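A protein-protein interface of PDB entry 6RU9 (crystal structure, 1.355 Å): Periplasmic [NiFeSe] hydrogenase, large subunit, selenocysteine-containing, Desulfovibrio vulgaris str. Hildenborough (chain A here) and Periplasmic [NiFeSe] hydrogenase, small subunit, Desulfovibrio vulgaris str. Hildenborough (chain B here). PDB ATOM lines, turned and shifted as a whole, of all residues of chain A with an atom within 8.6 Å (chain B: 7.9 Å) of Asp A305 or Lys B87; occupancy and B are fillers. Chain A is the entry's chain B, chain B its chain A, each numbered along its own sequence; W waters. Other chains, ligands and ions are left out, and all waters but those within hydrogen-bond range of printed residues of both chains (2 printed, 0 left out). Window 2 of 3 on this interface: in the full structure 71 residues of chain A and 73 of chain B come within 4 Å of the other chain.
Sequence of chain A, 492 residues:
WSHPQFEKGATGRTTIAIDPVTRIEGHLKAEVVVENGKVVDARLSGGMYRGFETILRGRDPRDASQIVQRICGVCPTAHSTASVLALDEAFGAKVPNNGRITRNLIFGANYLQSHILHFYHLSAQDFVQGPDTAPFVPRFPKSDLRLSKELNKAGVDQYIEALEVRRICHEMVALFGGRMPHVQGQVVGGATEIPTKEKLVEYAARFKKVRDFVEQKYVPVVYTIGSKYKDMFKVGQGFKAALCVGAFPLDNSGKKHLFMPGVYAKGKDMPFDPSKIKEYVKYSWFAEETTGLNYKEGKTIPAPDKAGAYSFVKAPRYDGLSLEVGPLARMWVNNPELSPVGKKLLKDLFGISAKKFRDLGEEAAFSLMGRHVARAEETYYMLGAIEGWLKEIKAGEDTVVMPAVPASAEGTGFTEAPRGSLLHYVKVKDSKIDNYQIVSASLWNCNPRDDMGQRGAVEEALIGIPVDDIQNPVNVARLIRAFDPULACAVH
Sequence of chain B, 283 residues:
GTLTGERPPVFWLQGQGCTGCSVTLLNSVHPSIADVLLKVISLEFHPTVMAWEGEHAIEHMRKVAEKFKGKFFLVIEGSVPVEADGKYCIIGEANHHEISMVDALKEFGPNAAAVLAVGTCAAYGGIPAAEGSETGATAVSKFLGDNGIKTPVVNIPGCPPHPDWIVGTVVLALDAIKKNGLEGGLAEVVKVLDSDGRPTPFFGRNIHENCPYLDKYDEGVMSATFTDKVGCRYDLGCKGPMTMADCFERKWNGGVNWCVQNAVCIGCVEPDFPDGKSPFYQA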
ATOM      1  N   GLY A  46      -0.769  -5.806   2.795  1.00  0.00           N
ATOM      2  CA  GLY A  46       0.603  -6.286   2.792  1.00  0.00           C
ATOM      3  C   GLY A  46       0.551  -7.807   2.810  1.00  0.00           C
ATOM      4  O   GLY A  46       0.097  -8.402   3.785  1.00  0.00           O
ATOM      5  N   GLY A  47       0.982  -8.456   1.738  1.00  0.00           N
ATOM      6  CA  GLY A  47       0.740  -9.871   1.568  1.00  0.00           C
ATOM      7  C   GLY A  47       1.841 -10.843   1.924  1.00  0.00           C
ATOM      8  O   GLY A  47       1.680 -12.043   1.658  1.00  0.00           O
ATOM      9  N   MET A  48       2.926 -10.397   2.561  1.00  0.00           N
ATOM     10  CA  MET A  48       4.036 -11.282   2.923  1.00  0.00           C
ATOM     11  C   MET A  48       4.479 -11.014   4.355  1.00  0.00           C
ATOM     12  O   MET A  48       4.724  -9.874   4.736  1.00  0.00           O
ATOM     13  CB  MET A  48       5.215 -11.130   1.963  1.00  0.00           C
ATOM     14  CG  MET A  48       6.360 -12.113   2.170  1.00  0.00           C
ATOM     15  SD  MET A  48       7.563 -11.620   3.421  1.00  0.00           S
ATOM     16  CE  MET A  48       8.537 -10.393   2.570  1.00  0.00           C
ATOM     17  N   TYR A  49       4.637 -12.090   5.119  1.00  0.00           N
ATOM     18  CA  TYR A  49       5.020 -12.035   6.520  1.00  0.00           C
ATOM     19  C   TYR A  49       6.212 -12.947   6.775  1.00  0.00           C
ATOM     20  O   TYR A  49       6.281 -14.066   6.246  1.00  0.00           O
ATOM     21  CB  TYR A  49       3.877 -12.509   7.362  1.00  0.00           C
ATOM     22  CG  TYR A  49       4.147 -12.622   8.842  1.00  0.00           C
ATOM     23  CD1 TYR A  49       4.110 -11.509   9.656  1.00  0.00           C
ATOM     24  CD2 TYR A  49       4.426 -13.846   9.421  1.00  0.00           C
ATOM     25  CE1 TYR A  49       4.356 -11.618  11.033  1.00  0.00           C
ATOM     26  CE2 TYR A  49       4.642 -13.971  10.792  1.00  0.00           C
ATOM     27  CZ  TYR A  49       4.616 -12.851  11.585  1.00  0.00           C
ATOM     28  OH  TYR A  49       4.823 -12.949  12.944  1.00  0.00           O
ATOM     29  N   SER A 284      -6.066  -6.847  10.542  1.00  0.00           N
ATOM     30  CA  SER A 284      -4.753  -7.416  10.290  1.00  0.00           C
ATOM     31  C   SER A 284      -4.746  -8.872  10.726  1.00  0.00           C
ATOM     32  O   SER A 284      -5.492  -9.250  11.623  1.00  0.00           O
ATOM     33  CB  SER A 284      -3.667  -6.657  11.072  1.00  0.00           C
ATOM     34  OG  SER A 284      -3.745  -5.238  10.900  1.00  0.00           O
ATOM     35  N   TRP A 285      -3.901  -9.685  10.078  1.00  0.00           N
ATOM     36  CA  TRP A 285      -3.850 -11.124  10.315  1.00  0.00           C
ATOM     37  C   TRP A 285      -3.029 -11.465  11.566  1.00  0.00           C
ATOM     38  O   TRP A 285      -2.005 -12.155  11.506  1.00  0.00           O
ATOM     39  CB  TRP A 285      -3.320 -11.858   9.084  1.00  0.00           C
ATOM     40  CG  TRP A 285      -4.309 -11.903   7.925  1.00  0.00           C
ATOM     41  CD1 TRP A 285      -5.593 -12.351   7.960  1.00  0.00           C
ATOM     42  CD2 TRP A 285      -4.070 -11.463   6.577  1.00  0.00           C
ATOM     43  NE1 TRP A 285      -6.180 -12.203   6.726  1.00  0.00           N
ATOM     44  CE2 TRP A 285      -5.259 -11.670   5.860  1.00  0.00           C
ATOM     45  CE3 TRP A 285      -2.965 -10.909   5.917  1.00  0.00           C
ATOM     46  CZ2 TRP A 285      -5.377 -11.352   4.512  1.00  0.00           C
ATOM     47  CZ3 TRP A 285      -3.074 -10.606   4.572  1.00  0.00           C
ATOM     48  CH2 TRP A 285      -4.289 -10.828   3.890  1.00  0.00           C
ATOM     49  N   PHE A 286      -3.521 -10.985  12.716  1.00  0.00           N
ATOM     50  CA  PHE A 286      -2.955 -11.246  14.035  1.00  0.00           C
ATOM     51  C   PHE A 286      -4.079 -11.531  15.011  1.00  0.00           C
ATOM     52  O   PHE A 286      -5.220 -11.100  14.815  1.00  0.00           O
ATOM     53  CB  PHE A 286      -2.073 -10.085  14.515  1.00  0.00           C
ATOM     54  CG  PHE A 286      -0.943  -9.806  13.587  1.00  0.00           C
ATOM     55  CD1 PHE A 286       0.179 -10.605  13.613  1.00  0.00           C
ATOM     56  CD2 PHE A 286      -1.050  -8.846  12.591  1.00  0.00           C
ATOM     57  CE1 PHE A 286       1.207 -10.420  12.724  1.00  0.00           C
ATOM     58  CE2 PHE A 286      -0.017  -8.652  11.685  1.00  0.00           C
ATOM     59  CZ  PHE A 286       1.101  -9.439  11.750  1.00  0.00           C
ATOM     60  N   PRO A 302       0.539 -14.400  14.656  1.00  0.00           N
ATOM     61  CA  PRO A 302      -0.136 -14.395  13.355  1.00  0.00           C
ATOM     62  C   PRO A 302      -1.429 -15.191  13.389  1.00  0.00           C
ATOM     63  O   PRO A 302      -1.587 -16.160  14.130  1.00  0.00           O
ATOM     64  CB  PRO A 302       0.894 -15.007  12.394  1.00  0.00           C
ATOM     65  CG  PRO A 302       1.998 -15.521  13.227  1.00  0.00           C
ATOM     66  CD  PRO A 302       1.910 -14.939  14.591  1.00  0.00           C
ATOM     67  N   ALA A 303      -2.383 -14.722  12.606  1.00  0.00           N
ATOM     68  CA  ALA A 303      -3.698 -15.339  12.478  1.00  0.00           C
ATOM     69  C   ALA A 303      -4.097 -15.187  11.019  1.00  0.00           C
ATOM     70  O   ALA A 303      -4.967 -14.375  10.679  1.00  0.00           O
ATOM     71  CB  ALA A 303      -4.708 -14.678  13.412  1.00  0.00           C
ATOM     72  N   PRO A 304      -3.467 -15.953  10.119  1.00  0.00           N
ATOM     73  CA  PRO A 304      -3.683 -15.728   8.683  1.00  0.00           C
ATOM     74  C   PRO A 304      -5.066 -16.092   8.190  1.00  0.00           C
ATOM     75  O   PRO A 304      -5.386 -15.752   7.034  1.00  0.00           O
ATOM     76  CB  PRO A 304      -2.610 -16.611   8.010  1.00  0.00           C
ATOM     77  CG  PRO A 304      -2.319 -17.667   9.006  1.00  0.00           C
ATOM     78  CD  PRO A 304      -2.487 -17.028  10.373  1.00  0.00           C
ATOM     79  N   ASP A 305      -5.876 -16.766   8.999  1.00  0.00           N
ATOM     80  CA  ASP A 305      -7.219 -17.152   8.615  1.00  0.00           C
ATOM     81  C   ASP A 305      -8.282 -16.282   9.272  1.00  0.00           C
ATOM     82  O   ASP A 305      -9.480 -16.549   9.104  1.00  0.00           O
ATOM     83  CB  ASP A 305      -7.466 -18.625   8.970  1.00  0.00           C
ATOM     84  CG  ASP A 305      -6.566 -19.581   8.199  1.00  0.00           C
ATOM     85  OD1 ASP A 305      -6.234 -19.304   7.035  1.00  0.00           O
ATOM     86  OD2 ASP A 305      -6.200 -20.626   8.766  1.00  0.00           O
ATOM     87  N   LYS A 306      -7.886 -15.238   9.992  1.00  0.00           N
ATOM     88  CA  LYS A 306      -8.861 -14.471  10.756  1.00  0.00           C
ATOM     89  C   LYS A 306      -9.839 -13.741   9.841  1.00  0.00           C
ATOM     90  O   LYS A 306      -9.426 -12.994   8.942  1.00  0.00           O
ATOM     91  CB  LYS A 306      -8.177 -13.478  11.687  1.00  0.00           C
ATOM     92  CG  LYS A 306      -9.160 -12.812  12.635  1.00  0.00           C
ATOM     93  CD  LYS A 306      -8.496 -11.831  13.595  1.00  0.00           C
ATOM     94  CE  LYS A 306      -8.055 -10.555  12.903  1.00  0.00           C
ATOM     95  NZ  LYS A 306      -7.390  -9.654  13.864  1.00  0.00           N
ATOM     96  N   ALA A 307     -11.136 -13.939  10.096  1.00  0.00           N
ATOM     97  CA  ALA A 307     -12.167 -13.370   9.237  1.00  0.00           C
ATOM     98  C   ALA A 307     -12.122 -11.844   9.254  1.00  0.00           C
ATOM     99  O   ALA A 307     -11.946 -11.208  10.301  1.00  0.00           O
ATOM    100  CB  ALA A 307     -13.552 -13.862   9.680  1.00  0.00           C
ATOM    101  N   GLY A 308     -12.279 -11.246   8.069  1.00  0.00           N
ATOM    102  CA  GLY A 308     -12.351  -9.815   7.948  1.00  0.00           C
ATOM    103  C   GLY A 308     -11.023  -9.099   7.815  1.00  0.00           C
ATOM    104  O   GLY A 308     -10.997  -7.949   7.360  1.00  0.00           O
ATOM    105  N   ALA A 309      -9.924  -9.730   8.204  1.00  0.00           N
ATOM    106  CA  ALA A 309      -8.624  -9.106   8.093  1.00  0.00           C
ATOM    107  C   ALA A 309      -8.157  -9.137   6.643  1.00  0.00           C
ATOM    108  O   ALA A 309      -8.588  -9.972   5.850  1.00  0.00           O
ATOM    109  CB  ALA A 309      -7.645  -9.829   9.015  1.00  0.00           C
ATOM    110  N   SER A 311      -4.560  -7.769   5.847  1.00  0.00           N
ATOM    111  CA  SER A 311      -3.163  -7.357   5.703  1.00  0.00           C
ATOM    112  C   SER A 311      -2.335  -7.926   6.832  1.00  0.00           C
ATOM    113  O   SER A 311      -2.846  -8.124   7.936  1.00  0.00           O
ATOM    114  CB  SER A 311      -3.051  -5.826   5.737  1.00  0.00           C
ATOM    115  OG  SER A 311      -1.721  -5.399   5.489  1.00  0.00           O
ATOM    116  N   PHE A 312      -1.060  -8.154   6.551  1.00  0.00           N
ATOM    117  CA  PHE A 312      -0.089  -8.472   7.590  1.00  0.00           C
ATOM    118  C   PHE A 312       0.515  -7.234   8.252  1.00  0.00           C
ATOM    119  O   PHE A 312       1.348  -7.369   9.169  1.00  0.00           O
ATOM    120  CB  PHE A 312       1.043  -9.363   7.060  1.00  0.00           C
ATOM    121  CG  PHE A 312       0.621 -10.798   6.817  1.00  0.00           C
ATOM    122  CD1 PHE A 312       0.243 -11.624   7.861  1.00  0.00           C
ATOM    123  CD2 PHE A 312       0.609 -11.304   5.538  1.00  0.00           C
ATOM    124  CE1 PHE A 312      -0.123 -12.940   7.620  1.00  0.00           C
ATOM    125  CE2 PHE A 312       0.232 -12.609   5.279  1.00  0.00           C
ATOM    126  CZ  PHE A 312      -0.119 -13.437   6.309  1.00  0.00           C
ATOM    127  N   PRO B  81       7.266 -19.814   1.832  1.00  0.00           N
ATOM    128  CA  PRO B  81       6.591 -20.305   3.035  1.00  0.00           C
ATOM    129  C   PRO B  81       5.434 -21.215   2.695  1.00  0.00           C
ATOM    130  O   PRO B  81       4.542 -20.866   1.900  1.00  0.00           O
ATOM    131  CB  PRO B  81       6.120 -19.027   3.737  1.00  0.00           C
ATOM    132  CG  PRO B  81       5.864 -18.062   2.598  1.00  0.00           C
ATOM    133  CD  PRO B  81       6.817 -18.451   1.466  1.00  0.00           C
ATOM    134  N   VAL B  82       5.438 -22.407   3.292  1.00  0.00           N
ATOM    135  CA  VAL B  82       4.426 -23.412   2.964  1.00  0.00           C
ATOM    136  C   VAL B  82       3.286 -23.501   3.977  1.00  0.00           C
ATOM    137  O   VAL B  82       2.247 -24.109   3.650  1.00  0.00           O
ATOM    138  CB  VAL B  82       5.055 -24.816   2.746  1.00  0.00           C
ATOM    139  CG1 VAL B  82       6.082 -24.761   1.625  1.00  0.00           C
ATOM    140  CG2 VAL B  82       5.661 -25.315   4.055  1.00  0.00           C
ATOM    141  N   GLU B  83       3.418 -22.925   5.169  1.00  0.00           N
ATOM    142  CA  GLU B  83       2.372 -23.027   6.178  1.00  0.00           C
ATOM    143  C   GLU B  83       1.146 -22.215   5.766  1.00  0.00           C
ATOM    144  O   GLU B  83       1.202 -21.340   4.901  1.00  0.00           O
ATOM    145  CB  GLU B  83       2.877 -22.541   7.541  1.00  0.00           C
ATOM    146  CG  GLU B  83       3.901 -23.452   8.197  1.00  0.00           C
ATOM    147  CD  GLU B  83       3.341 -24.821   8.579  1.00  0.00           C
ATOM    148  OE1 GLU B  83       2.094 -24.961   8.739  1.00  0.00           O
ATOM    149  OE2 GLU B  83       4.156 -25.766   8.702  1.00  0.00           O
ATOM    150  N   ALA B  84       0.010 -22.550   6.371  1.00  0.00           N
ATOM    151  CA  ALA B  84      -1.232 -21.821   6.128  1.00  0.00           C
ATOM    152  C   ALA B  84      -1.585 -21.776   4.641  1.00  0.00           C
ATOM    153  O   ALA B  84      -2.039 -20.747   4.116  1.00  0.00           O
ATOM    154  CB  ALA B  84      -1.173 -20.426   6.737  1.00  0.00           C
ATOM    155  N   ASP B  85      -1.356 -22.892   3.945  1.00  0.00           N
ATOM    156  CA  ASP B  85      -1.712 -23.018   2.530  1.00  0.00           C
ATOM    157  C   ASP B  85      -1.063 -21.920   1.685  1.00  0.00           C
ATOM    158  O   ASP B  85      -1.654 -21.408   0.726  1.00  0.00           O
ATOM    159  CB  ASP B  85      -3.227 -23.052   2.322  1.00  0.00           C
ATOM    160  CG  ASP B  85      -3.605 -23.466   0.911  1.00  0.00           C
ATOM    161  OD1 ASP B  85      -2.937 -24.378   0.359  1.00  0.00           O
ATOM    162  OD2 ASP B  85      -4.569 -22.891   0.359  1.00  0.00           O
ATOM    163  N   GLY B  86       0.165 -21.548   2.046  1.00  0.00           N
ATOM    164  CA  GLY B  86       0.907 -20.575   1.279  1.00  0.00           C
ATOM    165  C   GLY B  86       0.570 -19.129   1.569  1.00  0.00           C
ATOM    166  O   GLY B  86       1.160 -18.247   0.950  1.00  0.00           O
ATOM    167  N   LYS B  87      -0.341 -18.857   2.514  1.00  0.00           N
ATOM    168  CA  LYS B  87      -0.865 -17.499   2.695  1.00  0.00           C
ATOM    169  C   LYS B  87       0.142 -16.508   3.271  1.00  0.00           C
ATOM    170  O   LYS B  87      -0.147 -15.294   3.292  1.00  0.00           O
ATOM    171  CB  LYS B  87      -2.094 -17.522   3.596  1.00  0.00           C
ATOM    172  CG  LYS B  87      -3.342 -18.099   2.972  1.00  0.00           C
ATOM    173  CD  LYS B  87      -4.456 -18.172   4.020  1.00  0.00           C
ATOM    174  CE  LYS B  87      -5.723 -18.804   3.462  1.00  0.00           C
ATOM    175  NZ  LYS B  87      -6.823 -18.713   4.469  1.00  0.00           N
ATOM    176  N   TYR B  88       1.291 -16.959   3.767  1.00  0.00           N
ATOM    177  CA  TYR B  88       2.272 -16.003   4.274  1.00  0.00           C
ATOM    178  C   TYR B  88       3.067 -15.323   3.170  1.00  0.00           C
ATOM    179  O   TYR B  88       3.920 -14.474   3.471  1.00  0.00           O
ATOM    180  CB  TYR B  88       3.231 -16.670   5.262  1.00  0.00           C
ATOM    181  CG  TYR B  88       2.591 -17.030   6.595  1.00  0.00           C
ATOM    182  CD1 TYR B  88       2.110 -16.038   7.443  1.00  0.00           C
ATOM    183  CD2 TYR B  88       2.487 -18.361   7.028  1.00  0.00           C
ATOM    184  CE1 TYR B  88       1.528 -16.339   8.651  1.00  0.00           C
ATOM    185  CE2 TYR B  88       1.922 -18.652   8.263  1.00  0.00           C
ATOM    186  CZ  TYR B  88       1.464 -17.623   9.075  1.00  0.00           C
ATOM    187  OH  TYR B  88       0.890 -17.886  10.289  1.00  0.00           O
ATOM    188  N   CYS B  89       2.821 -15.644   1.900  1.00  0.00           N
ATOM    189  CA  CYS B  89       3.444 -14.894   0.813  1.00  0.00           C
ATOM    190  C   CYS B  89       2.526 -14.945  -0.399  1.00  0.00           C
ATOM    191  O   CYS B  89       2.531 -15.926  -1.147  1.00  0.00           O
ATOM    192  CB  CYS B  89       4.830 -15.422   0.480  1.00  0.00           C
ATOM    193  SG  CYS B  89       5.683 -14.355  -0.693  1.00  0.00           S
ATOM    194  N   ILE B  90       1.738 -13.891  -0.578  1.00  0.00           N
ATOM    195  CA  ILE B  90       0.920 -13.709  -1.770  1.00  0.00           C
ATOM    196  C   ILE B  90       1.636 -12.710  -2.672  1.00  0.00           C
ATOM    197  O   ILE B  90       1.926 -11.581  -2.254  1.00  0.00           O
ATOM    198  CB  ILE B  90      -0.485 -13.211  -1.408  1.00  0.00           C
ATOM    199  CG1 ILE B  90      -1.217 -14.211  -0.516  1.00  0.00           C
ATOM    200  CG2 ILE B  90      -1.256 -12.890  -2.684  1.00  0.00           C
ATOM    201  CD1 ILE B  90      -1.308 -15.620  -1.056  1.00  0.00           C
ATOM    202  N   ILE B  91       1.917 -13.111  -3.912  1.00  0.00           N
ATOM    203  CA  ILE B  91       2.734 -12.311  -4.814  1.00  0.00           C
ATOM    204  C   ILE B  91       1.930 -11.632  -5.921  1.00  0.00           C
ATOM    205  O   ILE B  91       2.494 -10.823  -6.693  1.00  0.00           O
ATOM    206  CB  ILE B  91       3.890 -13.130  -5.422  1.00  0.00           C
ATOM    207  CG1 ILE B  91       3.378 -14.154  -6.413  1.00  0.00           C
ATOM    208  CG2 ILE B  91       4.689 -13.836  -4.346  1.00  0.00           C
ATOM    209  CD1 ILE B  91       4.469 -14.605  -7.400  1.00  0.00           C
ATOM    210  N   GLU B  98      -5.885 -15.268  -6.176  1.00  0.00           N
ATOM    211  CA  GLU B  98      -4.622 -14.929  -5.551  1.00  0.00           C
ATOM    212  C   GLU B  98      -3.568 -15.947  -5.953  1.00  0.00           C
ATOM    213  O   GLU B  98      -3.854 -17.125  -6.182  1.00  0.00           O
ATOM    214  CB  GLU B  98      -4.758 -14.919  -4.035  1.00  0.00           C
ATOM    215  CG  GLU B  98      -5.797 -13.970  -3.507  1.00  0.00           C
ATOM    216  CD  GLU B  98      -6.093 -14.209  -2.042  1.00  0.00           C
ATOM    217  OE1 GLU B  98      -7.131 -13.719  -1.550  1.00  0.00           O
ATOM    218  OE2 GLU B  98      -5.286 -14.897  -1.389  1.00  0.00           O
ATOM    219  N   SER B 100      -0.065 -17.418  -4.571  1.00  0.00           N
ATOM    220  CA  SER B 100       0.945 -17.497  -3.528  1.00  0.00           C
ATOM    221  C   SER B 100       2.320 -17.805  -4.128  1.00  0.00           C
ATOM    222  O   SER B 100       2.464 -18.193  -5.287  1.00  0.00           O
ATOM    223  CB  SER B 100       0.582 -18.585  -2.525  1.00  0.00           C
ATOM    224  OG  SER B 100       0.690 -19.846  -3.171  1.00  0.00           O
ATOM    225  N   MET B 101       3.360 -17.643  -3.306  1.00  0.00           N
ATOM    226  CA  MET B 101       4.687 -18.044  -3.766  1.00  0.00           C
ATOM    227  C   MET B 101       4.739 -19.539  -4.052  1.00  0.00           C
ATOM    228  O   MET B 101       5.371 -19.971  -5.026  1.00  0.00           O
ATOM    229  CB  MET B 101       5.740 -17.667  -2.745  1.00  0.00           C
ATOM    230  CG  MET B 101       7.157 -17.882  -3.219  1.00  0.00           C
ATOM    231  SD  MET B 101       7.589 -16.739  -4.591  1.00  0.00           S
ATOM    232  CE  MET B 101       9.282 -17.217  -4.885  1.00  0.00           C
ATOM    233  N   VAL B 102       4.070 -20.335  -3.218  1.00  0.00           N
ATOM    234  CA  VAL B 102       3.929 -21.765  -3.492  1.00  0.00           C
ATOM    235  C   VAL B 102       3.345 -21.984  -4.885  1.00  0.00           C
ATOM    236  O   VAL B 102       3.895 -22.756  -5.687  1.00  0.00           O
ATOM    237  CB  VAL B 102       3.077 -22.426  -2.396  1.00  0.00           C
ATOM    238  CG1 VAL B 102       2.631 -23.825  -2.830  1.00  0.00           C
ATOM    239  CG2 VAL B 102       3.844 -22.468  -1.073  1.00  0.00           C
ATOM    240  N   THR B 135       6.423 -19.715   9.638  1.00  0.00           N
ATOM    241  CA  THR B 135       5.749 -19.669   8.354  1.00  0.00           C
ATOM    242  C   THR B 135       6.056 -20.859   7.465  1.00  0.00           C
ATOM    243  O   THR B 135       5.554 -20.910   6.339  1.00  0.00           O
ATOM    244  CB  THR B 135       6.095 -18.390   7.586  1.00  0.00           C
ATOM    245  OG1 THR B 135       7.485 -18.385   7.243  1.00  0.00           O
ATOM    246  CG2 THR B 135       5.770 -17.155   8.419  1.00  0.00           C
HETATM  247  O   HOH W   1      -7.359 -15.523   5.079  1.00  0.00           O
HETATM  248  O   HOH W   2      -4.448 -21.506   6.069  1.00  0.00           O
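The side-chain amino group (NZ) of Lys B87 lies within salt-bridge range of the side-chain carboxylate (OD1) of Asp A305 (2.7 Å). The backbone carbonyl oxygen (O) of Tyr B88 is in hydrogen-bond range of the backbone NH (N) of Tyr A49 (3.0 Å). The backbone NH of Ile B90 lies within hydrogen-bond range of the backbone carbonyl oxygen of Gly A47 (2.9 Å).
O of Thr B135 sits at hydrogen-bond distance from N of Val B82, 3.4 Å away. The backbone NH of Glu B83 lies within hydrogen-bond range of the backbone carbonyl oxygen of Thr B135 (3.2 Å). The backbone carbonyl oxygen of Cys B89 is in hydrogen-bond range of the backbone NH of Met B101 (2.9 Å). O of Gly A46 is in hydrogen-bond range of N of Phe A312 (3.0 Å).
Among the printed residues, merely in contact across the chains: Gly A47 with Tyr B88 (3.8 Å), Gly A47 with Cys B89 (3.5 Å), Met A48 with Tyr B88 (3.2 Å), Met A48 with Cys B89 (3.7 Å), Tyr A49 with Thr B135 (3.7 Å), Pro A302 with Tyr B88 (3.6 Å), Pro A304 with Ala B84 (3.8 Å), Pro A304 with Lys B87 (3.98 Å), Pro A304 with Tyr B88 (3.5 Å), Phe A312 with Lys B87 (3.4 Å) and Phe A312 with Tyr B88 (3.6 Å).
Asp A305 touches just one residue of chain B: Lys B87 (2.7 Å). Of chain A, only Pro A304 (3.98 Å), Asp A305 (2.7 Å) and Phe A312 (3.4 Å) come within 4 Å of Lys B87. Pro A304 touches three residues of chain B. No residue of chain A comes within 4 Å of Gly B86. Of the printed residues of chain A, Tyr B88 touches Gly A47 (3.8 Å), Met A48 (3.2 Å), Tyr A49 (3.0 Å), Pro A302 (3.6 Å), Pro A304 (3.5 Å) and Phe A312 (3.6 Å). Of the printed residues of chain B, Met A48 touches Tyr B88 (3.2 Å) and Cys B89 (3.7 Å). Of the printed residues of chain A, Ala B84 touches Pro A304 (3.8 Å). Ile B91 touches none of the printed residues of chain A. The nearest residue of chain B that does not touch Asp A305 is Ala B84 (5.2 Å). The nearest printed residue of chain B that does not touch Tyr A49 is Cys B89 (5.1 Å).
Printed residues of chain A that touch a printed residue of chain B: Gly A47, Met A48, Tyr A49, Pro A302, Pro A304, Asp A305 and Phe A312. Hydrophobic or aromatic side chains of chain A that line the printed part of chain B: Met A48, Tyr A49, Pro A302, Pro A304 and Phe A312. Printed residues of chain B that touch a printed residue of chain A: Ala B84, Lys B87, Tyr B88, Cys B89, Ile B90 and Thr B135. Hydrophobic or aromatic side chains of chain B within 4 Å of the printed part of chain A: Ala B84, Tyr B88 and Ile B90. Along chain B the printed residues that touch a printed residue of chain A span positions 84 to 135. Among the printed residues, 14 pairs touch across the chains.
Water W1 bridges the backbone carbonyl oxygen (O) of Pro A304 (2.8 Å) and the side-chain amino group (NZ) of Lys B87 (3.3 Å). Water W2 lies within hydrogen-bond range of the side-chain carboxylate (OD1) of Asp A305 (3.0 Å) and the backbone carbonyl oxygen (O) of Ala B84 (3.2 Å).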
